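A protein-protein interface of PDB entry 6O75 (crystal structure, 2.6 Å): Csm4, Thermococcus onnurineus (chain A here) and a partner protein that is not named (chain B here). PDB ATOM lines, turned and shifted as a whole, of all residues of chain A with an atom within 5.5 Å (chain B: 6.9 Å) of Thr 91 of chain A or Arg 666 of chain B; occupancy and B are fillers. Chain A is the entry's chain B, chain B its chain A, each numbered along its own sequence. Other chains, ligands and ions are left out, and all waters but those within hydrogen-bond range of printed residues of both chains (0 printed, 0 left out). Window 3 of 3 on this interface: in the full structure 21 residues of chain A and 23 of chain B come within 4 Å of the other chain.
The guanidinium group (NH1) of Arg 538 of chain B sits at hydrogen-bond distance from the side-chain hydroxyl (OG1) of Thr 91 of chain A (2.8 Å).
NE of Arg 538 of chain B is in salt-bridge range of OE1 of Glu 87 of chain A (3.5 Å).
The guanidinium group (NE) of Arg 95 of chain A lies within salt-bridge range of the side-chain carboxylate (OD2) of Asp 663 of chain B.
O of Asp 659 of chain B lies within hydrogen-bond range of NH2 of Arg 95 of chain A (3.4 Å).
The backbone carbonyl oxygen (O) of Glu 87 of chain A sits at hydrogen-bond distance from the side-chain hydroxyl (OG1) of Thr 91 of chain A, 3.4 Å away.
O of Lys 662 of chain B sits at hydrogen-bond distance from NH2 of Arg 666 of chain B (3.2 Å).
Thr 91 of chain A touches Arg 666 of chain B (OG1 to NH2, 3.9 Å).
Of the printed residues of chain B, Glu 87 of chain A touches Arg 538 (3.4 Å).
Of the printed residues of chain B, Thr 91 of chain A touches Arg 538 (2.8 Å) and Arg 666 (3.9 Å).
Printed residues of chain A within 4 Å of Asp 659 of chain B: Arg 95 (3.4 Å).
Printed residues of chain A within 4 Å of Asp 663 of chain B: Arg 95.
Arg 666 of chain B touches just one residue of chain A: Thr 91 (3.9 Å).
Asn 667 of chain B touches none of the printed residues of chain A.
Arg 668 of chain B touches none of the printed residues of chain A.
Among the printed residues, 5 pairs touch across the chains.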
ATOM      1  N   GLU A  86       0.861 -31.690  12.990  1.00  0.00           N
ATOM      2  CA  GLU A  86      -0.089 -30.588  13.315  1.00  0.00           C
ATOM      3  C   GLU A  86      -0.961 -30.293  12.088  1.00  0.00           C
ATOM      4  O   GLU A  86      -2.192 -30.409  12.206  1.00  0.00           O
ATOM      5  CB  GLU A  86       0.649 -29.319  13.752  1.00  0.00           C
ATOM      6  CG  GLU A  86       1.130 -29.341  15.194  1.00  0.00           C
ATOM      7  CD  GLU A  86       1.889 -28.099  15.638  1.00  0.00           C
ATOM      8  OE1 GLU A  86       1.877 -27.095  14.896  1.00  0.00           O
ATOM      9  OE2 GLU A  86       2.492 -28.137  16.728  1.00  0.00           O
ATOM     10  N   GLU A  87      -0.336 -29.934  10.959  1.00  0.00           N
ATOM     11  CA  GLU A  87      -1.017 -29.489   9.707  1.00  0.00           C
ATOM     12  C   GLU A  87      -1.804 -30.648   9.075  1.00  0.00           C
ATOM     13  O   GLU A  87      -2.900 -30.383   8.540  1.00  0.00           O
ATOM     14  CB  GLU A  87      -0.017 -28.923   8.694  1.00  0.00           C
ATOM     15  CG  GLU A  87       0.008 -27.401   8.641  1.00  0.00           C
ATOM     16  CD  GLU A  87       0.570 -26.785   7.365  1.00  0.00           C
ATOM     17  OE1 GLU A  87       0.770 -25.554   7.352  1.00  0.00           O
ATOM     18  OE2 GLU A  87       0.798 -27.527   6.386  1.00  0.00           O
ATOM     19  N   GLU A  88      -1.265 -31.871   9.112  1.00  0.00           N
ATOM     20  CA  GLU A  88      -1.901 -33.081   8.522  1.00  0.00           C
ATOM     21  C   GLU A  88      -3.193 -33.423   9.274  1.00  0.00           C
ATOM     22  O   GLU A  88      -4.165 -33.820   8.603  1.00  0.00           O
ATOM     23  CB  GLU A  88      -0.958 -34.288   8.561  1.00  0.00           C
ATOM     24  CG  GLU A  88       0.101 -34.275   7.476  1.00  0.00           C
ATOM     25  CD  GLU A  88      -0.419 -34.615   6.090  1.00  0.00           C
ATOM     26  OE1 GLU A  88      -1.288 -33.874   5.586  1.00  0.00           O
ATOM     27  OE2 GLU A  88       0.040 -35.627   5.522  1.00  0.00           O
ATOM     28  N   ARG A  89      -3.200 -33.278  10.605  1.00  0.00           N
ATOM     29  CA  ARG A  89      -4.291 -33.784  11.484  1.00  0.00           C
ATOM     30  C   ARG A  89      -5.525 -32.880  11.338  1.00  0.00           C
ATOM     31  O   ARG A  89      -6.632 -33.436  11.234  1.00  0.00           O
ATOM     32  CB  ARG A  89      -3.788 -33.981  12.923  1.00  0.00           C
ATOM     33  CG  ARG A  89      -4.147 -32.894  13.931  1.00  0.00           C
ATOM     34  CD  ARG A  89      -4.634 -33.447  15.263  1.00  0.00           C
ATOM     35  NE  ARG A  89      -6.091 -33.451  15.352  1.00  0.00           N
ATOM     36  CZ  ARG A  89      -6.901 -34.429  14.939  1.00  0.00           C
ATOM     37  NH1 ARG A  89      -8.211 -34.295  15.075  1.00  0.00           N
ATOM     38  NH2 ARG A  89      -6.420 -35.536  14.397  1.00  0.00           N
ATOM     39  N   TYR A  90      -5.349 -31.553  11.292  1.00  0.00           N
ATOM     40  CA  TYR A  90      -6.454 -30.567  11.129  1.00  0.00           C
ATOM     41  C   TYR A  90      -7.060 -30.701   9.722  1.00  0.00           C
ATOM     42  O   TYR A  90      -8.270 -30.445   9.574  1.00  0.00           O
ATOM     43  CB  TYR A  90      -5.986 -29.129  11.384  1.00  0.00           C
ATOM     44  CG  TYR A  90      -5.317 -28.877  12.716  1.00  0.00           C
ATOM     45  CD1 TYR A  90      -5.961 -29.150  13.914  1.00  0.00           C
ATOM     46  CD2 TYR A  90      -4.042 -28.332  12.781  1.00  0.00           C
ATOM     47  CE1 TYR A  90      -5.348 -28.913  15.136  1.00  0.00           C
ATOM     48  CE2 TYR A  90      -3.415 -28.090  13.994  1.00  0.00           C
ATOM     49  CZ  TYR A  90      -4.072 -28.381  15.176  1.00  0.00           C
ATOM     50  OH  TYR A  90      -3.465 -28.143  16.374  1.00  0.00           O
ATOM     51  N   THR A  91      -6.251 -31.102   8.730  1.00  0.00           N
ATOM     52  CA  THR A  91      -6.635 -31.194   7.292  1.00  0.00           C
ATOM     53  C   THR A  91      -7.458 -32.466   7.047  1.00  0.00           C
ATOM     54  O   THR A  91      -8.509 -32.360   6.382  1.00  0.00           O
ATOM     55  CB  THR A  91      -5.403 -31.097   6.380  1.00  0.00           C
ATOM     56  OG1 THR A  91      -5.176 -29.706   6.149  1.00  0.00           O
ATOM     57  CG2 THR A  91      -5.559 -31.805   5.051  1.00  0.00           C
ATOM     58  N   THR A  92      -6.994 -33.620   7.536  1.00  0.00           N
ATOM     59  CA  THR A  92      -7.744 -34.905   7.493  1.00  0.00           C
ATOM     60  C   THR A  92      -9.042 -34.739   8.293  1.00  0.00           C
ATOM     61  O   THR A  92     -10.109 -35.061   7.743  1.00  0.00           O
ATOM     62  CB  THR A  92      -6.908 -36.087   8.009  1.00  0.00           C
ATOM     63  OG1 THR A  92      -6.072 -35.615   9.065  1.00  0.00           O
ATOM     64  CG2 THR A  92      -6.057 -36.731   6.936  1.00  0.00           C
ATOM     65  N   ALA A  93      -8.944 -34.213   9.520  1.00  0.00           N
ATOM     66  CA  ALA A  93     -10.061 -34.036  10.483  1.00  0.00           C
ATOM     67  C   ALA A  93     -11.208 -33.228   9.861  1.00  0.00           C
ATOM     68  O   ALA A  93     -12.365 -33.498  10.227  1.00  0.00           O
ATOM     69  CB  ALA A  93      -9.564 -33.373  11.743  1.00  0.00           C
ATOM     70  N   LYS A  94     -10.901 -32.265   8.986  1.00  0.00           N
ATOM     71  CA  LYS A  94     -11.912 -31.442   8.264  1.00  0.00           C
ATOM     72  C   LYS A  94     -12.617 -32.307   7.207  1.00  0.00           C
ATOM     73  O   LYS A  94     -13.823 -32.079   6.994  1.00  0.00           O
ATOM     74  CB  LYS A  94     -11.262 -30.200   7.640  1.00  0.00           C
ATOM     75  CG  LYS A  94     -12.230 -29.114   7.176  1.00  0.00           C
ATOM     76  CD  LYS A  94     -12.642 -28.126   8.260  1.00  0.00           C
ATOM     77  CE  LYS A  94     -12.065 -26.734   8.075  1.00  0.00           C
ATOM     78  NZ  LYS A  94     -10.611 -26.676   8.366  1.00  0.00           N
ATOM     79  N   ARG A  95     -11.910 -33.266   6.589  1.00  0.00           N
ATOM     80  CA  ARG A  95     -12.442 -34.155   5.511  1.00  0.00           C
ATOM     81  C   ARG A  95     -13.158 -35.374   6.108  1.00  0.00           C
ATOM     82  O   ARG A  95     -14.102 -35.872   5.459  1.00  0.00           O
ATOM     83  CB  ARG A  95     -11.333 -34.569   4.533  1.00  0.00           C
ATOM     84  CG  ARG A  95     -11.321 -33.769   3.233  1.00  0.00           C
ATOM     85  CD  ARG A  95     -11.679 -32.307   3.465  1.00  0.00           C
ATOM     86  NE  ARG A  95     -11.448 -31.383   2.359  1.00  0.00           N
ATOM     87  CZ  ARG A  95     -11.530 -30.054   2.465  1.00  0.00           C
ATOM     88  NH1 ARG A  95     -11.824 -29.492   3.627  1.00  0.00           N
ATOM     89  NH2 ARG A  95     -11.309 -29.279   1.418  1.00  0.00           N
ATOM     90  N   VAL B 536      -9.453 -17.250   4.092  1.00  0.00           N
ATOM     91  CA  VAL B 536      -8.021 -17.335   4.500  1.00  0.00           C
ATOM     92  C   VAL B 536      -7.691 -18.776   4.884  1.00  0.00           C
ATOM     93  O   VAL B 536      -8.522 -19.432   5.534  1.00  0.00           O
ATOM     94  CB  VAL B 536      -7.701 -16.351   5.642  1.00  0.00           C
ATOM     95  CG1 VAL B 536      -6.312 -16.589   6.228  1.00  0.00           C
ATOM     96  CG2 VAL B 536      -7.857 -14.919   5.157  1.00  0.00           C
ATOM     97  N   ASP B 537      -6.502 -19.229   4.504  1.00  0.00           N
ATOM     98  CA  ASP B 537      -6.014 -20.614   4.730  1.00  0.00           C
ATOM     99  C   ASP B 537      -5.418 -20.716   6.139  1.00  0.00           C
ATOM    100  O   ASP B 537      -4.653 -19.803   6.530  1.00  0.00           O
ATOM    101  CB  ASP B 537      -5.002 -20.988   3.646  1.00  0.00           C
ATOM    102  CG  ASP B 537      -5.537 -20.759   2.243  1.00  0.00           C
ATOM    103  OD1 ASP B 537      -6.660 -21.239   1.949  1.00  0.00           O
ATOM    104  OD2 ASP B 537      -4.842 -20.088   1.462  1.00  0.00           O
ATOM    105  N   ARG B 538      -5.808 -21.767   6.870  1.00  0.00           N
ATOM    106  CA  ARG B 538      -5.185 -22.272   8.124  1.00  0.00           C
ATOM    107  C   ARG B 538      -5.155 -21.176   9.196  1.00  0.00           C
ATOM    108  O   ARG B 538      -4.194 -21.149   9.988  1.00  0.00           O
ATOM    109  CB  ARG B 538      -3.793 -22.833   7.814  1.00  0.00           C
ATOM    110  CG  ARG B 538      -3.819 -24.024   6.867  1.00  0.00           C
ATOM    111  CD  ARG B 538      -2.565 -24.877   6.935  1.00  0.00           C
ATOM    112  NE  ARG B 538      -2.375 -25.644   5.712  1.00  0.00           N
ATOM    113  CZ  ARG B 538      -3.098 -26.701   5.346  1.00  0.00           C
ATOM    114  NH1 ARG B 538      -4.083 -27.146   6.110  1.00  0.00           N
ATOM    115  NH2 ARG B 538      -2.837 -27.309   4.201  1.00  0.00           N
ATOM    116  N   THR B 633      -2.111 -16.819   3.377  1.00  0.00           N
ATOM    117  CA  THR B 633      -2.632 -16.996   2.000  1.00  0.00           C
ATOM    118  C   THR B 633      -4.155 -17.136   2.022  1.00  0.00           C
ATOM    119  O   THR B 633      -4.703 -17.574   3.057  1.00  0.00           O
ATOM    120  CB  THR B 633      -1.971 -18.195   1.311  1.00  0.00           C
ATOM    121  OG1 THR B 633      -2.409 -19.387   1.957  1.00  0.00           O
ATOM    122  CG2 THR B 633      -0.461 -18.124   1.334  1.00  0.00           C
ATOM    123  N   LEU B 634      -4.781 -16.744   0.905  1.00  0.00           N
ATOM    124  CA  LEU B 634      -6.220 -16.915   0.576  1.00  0.00           C
ATOM    125  C   LEU B 634      -6.380 -18.102  -0.366  1.00  0.00           C
ATOM    126  O   LEU B 634      -5.462 -18.388  -1.129  1.00  0.00           O
ATOM    127  CB  LEU B 634      -6.746 -15.676  -0.161  1.00  0.00           C
ATOM    128  CG  LEU B 634      -6.763 -14.365   0.610  1.00  0.00           C
ATOM    129  CD1 LEU B 634      -7.383 -13.270  -0.238  1.00  0.00           C
ATOM    130  CD2 LEU B 634      -7.526 -14.513   1.910  1.00  0.00           C
ATOM    131  N   SER B 635      -7.559 -18.702  -0.361  1.00  0.00           N
ATOM    132  CA  SER B 635      -8.089 -19.484  -1.498  1.00  0.00           C
ATOM    133  C   SER B 635      -9.377 -18.805  -1.967  1.00  0.00           C
ATOM    134  O   SER B 635     -10.041 -18.149  -1.149  1.00  0.00           O
ATOM    135  CB  SER B 635      -8.253 -20.926  -1.120  1.00  0.00           C
ATOM    136  OG  SER B 635      -6.986 -21.476  -0.766  1.00  0.00           O
ATOM    137  N   ASP B 659     -13.867 -24.951  -1.792  1.00  0.00           N
ATOM    138  CA  ASP B 659     -13.515 -26.221  -1.103  1.00  0.00           C
ATOM    139  C   ASP B 659     -12.445 -26.940  -1.925  1.00  0.00           C
ATOM    140  O   ASP B 659     -11.442 -27.352  -1.338  1.00  0.00           O
ATOM    141  CB  ASP B 659     -14.745 -27.100  -0.871  1.00  0.00           C
ATOM    142  CG  ASP B 659     -15.668 -26.584   0.220  1.00  0.00           C
ATOM    143  OD1 ASP B 659     -16.854 -26.998   0.240  1.00  0.00           O
ATOM    144  OD2 ASP B 659     -15.201 -25.772   1.041  1.00  0.00           O
ATOM    145  N   ALA B 661     -10.311 -25.693  -4.227  1.00  0.00           N
ATOM    146  CA  ALA B 661      -9.068 -24.892  -4.137  1.00  0.00           C
ATOM    147  C   ALA B 661      -8.288 -25.292  -2.878  1.00  0.00           C
ATOM    148  O   ALA B 661      -7.074 -25.378  -2.967  1.00  0.00           O
ATOM    149  CB  ALA B 661      -9.378 -23.417  -4.154  1.00  0.00           C
ATOM    150  N   LYS B 662      -8.974 -25.572  -1.769  1.00  0.00           N
ATOM    151  CA  LYS B 662      -8.358 -25.930  -0.464  1.00  0.00           C
ATOM    152  C   LYS B 662      -7.910 -27.400  -0.467  1.00  0.00           C
ATOM    153  O   LYS B 662      -6.810 -27.658   0.054  1.00  0.00           O
ATOM    154  CB  LYS B 662      -9.323 -25.568   0.672  1.00  0.00           C
ATOM    155  CG  LYS B 662      -9.622 -24.074   0.755  1.00  0.00           C
ATOM    156  CD  LYS B 662     -10.056 -23.567   2.113  1.00  0.00           C
ATOM    157  CE  LYS B 662      -9.951 -22.059   2.207  1.00  0.00           C
ATOM    158  NZ  LYS B 662      -9.490 -21.605   3.537  1.00  0.00           N
ATOM    159  N   ASP B 663      -8.694 -28.324  -1.040  1.00  0.00           N
ATOM    160  CA  ASP B 663      -8.332 -29.767  -1.151  1.00  0.00           C
ATOM    161  C   ASP B 663      -7.004 -29.931  -1.898  1.00  0.00           C
ATOM    162  O   ASP B 663      -6.250 -30.845  -1.532  1.00  0.00           O
ATOM    163  CB  ASP B 663      -9.366 -30.589  -1.920  1.00  0.00           C
ATOM    164  CG  ASP B 663     -10.583 -30.990  -1.109  1.00  0.00           C
ATOM    165  OD1 ASP B 663     -10.771 -32.208  -0.890  1.00  0.00           O
ATOM    166  OD2 ASP B 663     -11.347 -30.086  -0.720  1.00  0.00           O
ATOM    167  N   GLU B 664      -6.748 -29.090  -2.908  1.00  0.00           N
ATOM    168  CA  GLU B 664      -5.639 -29.236  -3.891  1.00  0.00           C
ATOM    169  C   GLU B 664      -4.386 -28.492  -3.397  1.00  0.00           C
ATOM    170  O   GLU B 664      -3.506 -28.188  -4.222  1.00  0.00           O
ATOM    171  CB  GLU B 664      -6.106 -28.734  -5.261  1.00  0.00           C
ATOM    172  CG  GLU B 664      -7.349 -29.440  -5.774  1.00  0.00           C
ATOM    173  CD  GLU B 664      -7.740 -29.170  -7.220  1.00  0.00           C
ATOM    174  OE1 GLU B 664      -8.162 -30.126  -7.905  1.00  0.00           O
ATOM    175  OE2 GLU B 664      -7.638 -28.009  -7.656  1.00  0.00           O
ATOM    176  N   GLY B 665      -4.270 -28.284  -2.087  1.00  0.00           N
ATOM    177  CA  GLY B 665      -3.344 -27.315  -1.476  1.00  0.00           C
ATOM    178  C   GLY B 665      -4.109 -26.054  -1.149  1.00  0.00           C
ATOM    179  O   GLY B 665      -5.321 -26.028  -1.389  1.00  0.00           O
ATOM    180  N   ARG B 666      -3.452 -25.043  -0.608  1.00  0.00           N
ATOM    181  CA  ARG B 666      -4.100 -23.739  -0.327  1.00  0.00           C
ATOM    182  C   ARG B 666      -3.306 -22.692  -1.111  1.00  0.00           C
ATOM    183  O   ARG B 666      -2.488 -23.108  -1.954  1.00  0.00           O
ATOM    184  CB  ARG B 666      -4.214 -23.598   1.193  1.00  0.00           C
ATOM    185  CG  ARG B 666      -5.348 -24.435   1.775  1.00  0.00           C
ATOM    186  CD  ARG B 666      -5.150 -24.933   3.197  1.00  0.00           C
ATOM    187  NE  ARG B 666      -6.426 -25.259   3.836  1.00  0.00           N
ATOM    188  CZ  ARG B 666      -7.024 -26.458   3.830  1.00  0.00           C
ATOM    189  NH1 ARG B 666      -8.186 -26.621   4.444  1.00  0.00           N
ATOM    190  NH2 ARG B 666      -6.469 -27.489   3.221  1.00  0.00           N
ATOM    191  N   ASN B 667      -3.576 -21.401  -0.926  1.00  0.00           N
ATOM    192  CA  ASN B 667      -2.943 -20.340  -1.756  1.00  0.00           C
ATOM    193  C   ASN B 667      -3.219 -20.649  -3.237  1.00  0.00           C
ATOM    194  O   ASN B 667      -2.281 -20.550  -4.059  1.00  0.00           O
ATOM    195  CB  ASN B 667      -1.440 -20.241  -1.470  1.00  0.00           C
ATOM    196  CG  ASN B 667      -0.787 -18.996  -2.034  1.00  0.00           C
ATOM    197  OD1 ASN B 667      -1.384 -17.919  -2.069  1.00  0.00           O
ATOM    198  ND2 ASN B 667       0.454 -19.132  -2.464  1.00  0.00           N
ATOM    199  N   ARG B 668      -4.443 -21.064  -3.574  1.00  0.00           N
ATOM    200  CA  ARG B 668      -4.825 -21.298  -4.989  1.00  0.00           C
ATOM    201  C   ARG B 668      -6.228 -20.762  -5.257  1.00  0.00           C
ATOM    202  O   ARG B 668      -6.996 -20.539  -4.294  1.00  0.00           O
ATOM    203  CB  ARG B 668      -4.690 -22.760  -5.425  1.00  0.00           C
ATOM    204  CG  ARG B 668      -4.774 -23.814  -4.336  1.00  0.00           C
ATOM    205  CD  ARG B 668      -3.957 -25.036  -4.722  1.00  0.00           C
ATOM    206  NE  ARG B 668      -4.035 -25.325  -6.151  1.00  0.00           N
ATOM    207  CZ  ARG B 668      -3.040 -25.779  -6.914  1.00  0.00           C
ATOM    208  NH1 ARG B 668      -3.243 -25.989  -8.204  1.00  0.00           N
ATOM    209  NH2 ARG B 668      -1.845 -26.011  -6.404  1.00  0.00           N
ATOM    210  N   VAL B 669      -6.509 -20.534  -6.541  1.00  0.00           N
ATOM    211  CA  VAL B 669      -7.773 -19.924  -7.044  1.00  0.00           C
ATOM    212  C   VAL B 669      -8.368 -20.864  -8.092  1.00  0.00           C
ATOM    213  O   VAL B 669      -7.634 -21.314  -8.995  1.00  0.00           O
ATOM    214  CB  VAL B 669      -7.532 -18.510  -7.610  1.00  0.00           C
ATOM    215  CG1 VAL B 669      -6.491 -18.492  -8.721  1.00  0.00           C
ATOM    216  CG2 VAL B 669      -8.820 -17.851  -8.075  1.00  0.00           C
ATOM    217  N   TYR B 686      -5.603 -23.320  -9.708  1.00  0.00           N
ATOM    218  CA  TYR B 686      -4.222 -22.843  -9.970  1.00  0.00           C
ATOM    219  C   TYR B 686      -3.629 -22.249  -8.690  1.00  0.00           C
ATOM    220  O   TYR B 686      -4.366 -21.568  -7.980  1.00  0.00           O
ATOM    221  CB  TYR B 686      -4.213 -21.728 -11.013  1.00  0.00           C
ATOM    222  CG  TYR B 686      -4.621 -22.108 -12.412  1.00  0.00           C
ATOM    223  CD1 TYR B 686      -5.954 -22.281 -12.750  1.00  0.00           C
ATOM    224  CD2 TYR B 686      -3.670 -22.220 -13.417  1.00  0.00           C
ATOM    225  CE1 TYR B 686      -6.330 -22.614 -14.041  1.00  0.00           C
ATOM    226  CE2 TYR B 686      -4.032 -22.534 -14.716  1.00  0.00           C
ATOM    227  CZ  TYR B 686      -5.366 -22.733 -15.028  1.00  0.00           C
ATOM    228  OH  TYR B 686      -5.718 -23.048 -16.305  1.00  0.00           O
ATOM    229  N   GLU B 687      -2.329 -22.448  -8.446  1.00  0.00           N
ATOM    230  CA  GLU B 687      -1.538 -21.606  -7.507  1.00  0.00           C
ATOM    231  C   GLU B 687      -1.598 -20.175  -8.042  1.00  0.00           C
ATOM    232  O   GLU B 687      -1.404 -20.001  -9.265  1.00  0.00           O
ATOM    233  CB  GLU B 687      -0.057 -21.992  -7.425  1.00  0.00           C
ATOM    234  CG  GLU B 687       0.228 -23.456  -7.147  1.00  0.00           C
ATOM    235  CD  GLU B 687       1.521 -23.945  -7.787  1.00  0.00           C
ATOM    236  OE1 GLU B 687       1.527 -24.183  -9.022  1.00  0.00           O
ATOM    237  OE2 GLU B 687       2.531 -24.056  -7.061  1.00  0.00           O
ATOM    238  N   TRP B 688      -1.855 -19.197  -7.174  1.00  0.00           N
ATOM    239  CA  TRP B 688      -2.016 -17.774  -7.568  1.00  0.00           C
ATOM    240  C   TRP B 688      -0.879 -17.375  -8.509  1.00  0.00           C
ATOM    241  O   TRP B 688      -1.172 -16.790  -9.556  1.00  0.00           O
ATOM    242  CB  TRP B 688      -2.068 -16.862  -6.339  1.00  0.00           C
ATOM    243  CG  TRP B 688      -3.349 -16.921  -5.568  1.00  0.00           C
ATOM    244  CD1 TRP B 688      -3.562 -17.560  -4.381  1.00  0.00           C
ATOM    245  CD2 TRP B 688      -4.601 -16.301  -5.916  1.00  0.00           C
ATOM    246  NE1 TRP B 688      -4.854 -17.379  -3.964  1.00  0.00           N
ATOM    247  CE2 TRP B 688      -5.516 -16.613  -4.887  1.00  0.00           C
ATOM    248  CE3 TRP B 688      -5.042 -15.525  -6.995  1.00  0.00           C
ATOM    249  CZ2 TRP B 688      -6.829 -16.152  -4.893  1.00  0.00           C
ATOM    250  CZ3 TRP B 688      -6.346 -15.083  -7.008  1.00  0.00           C
ATOM    251  CH2 TRP B 688      -7.222 -15.388  -5.966  1.00  0.00           C
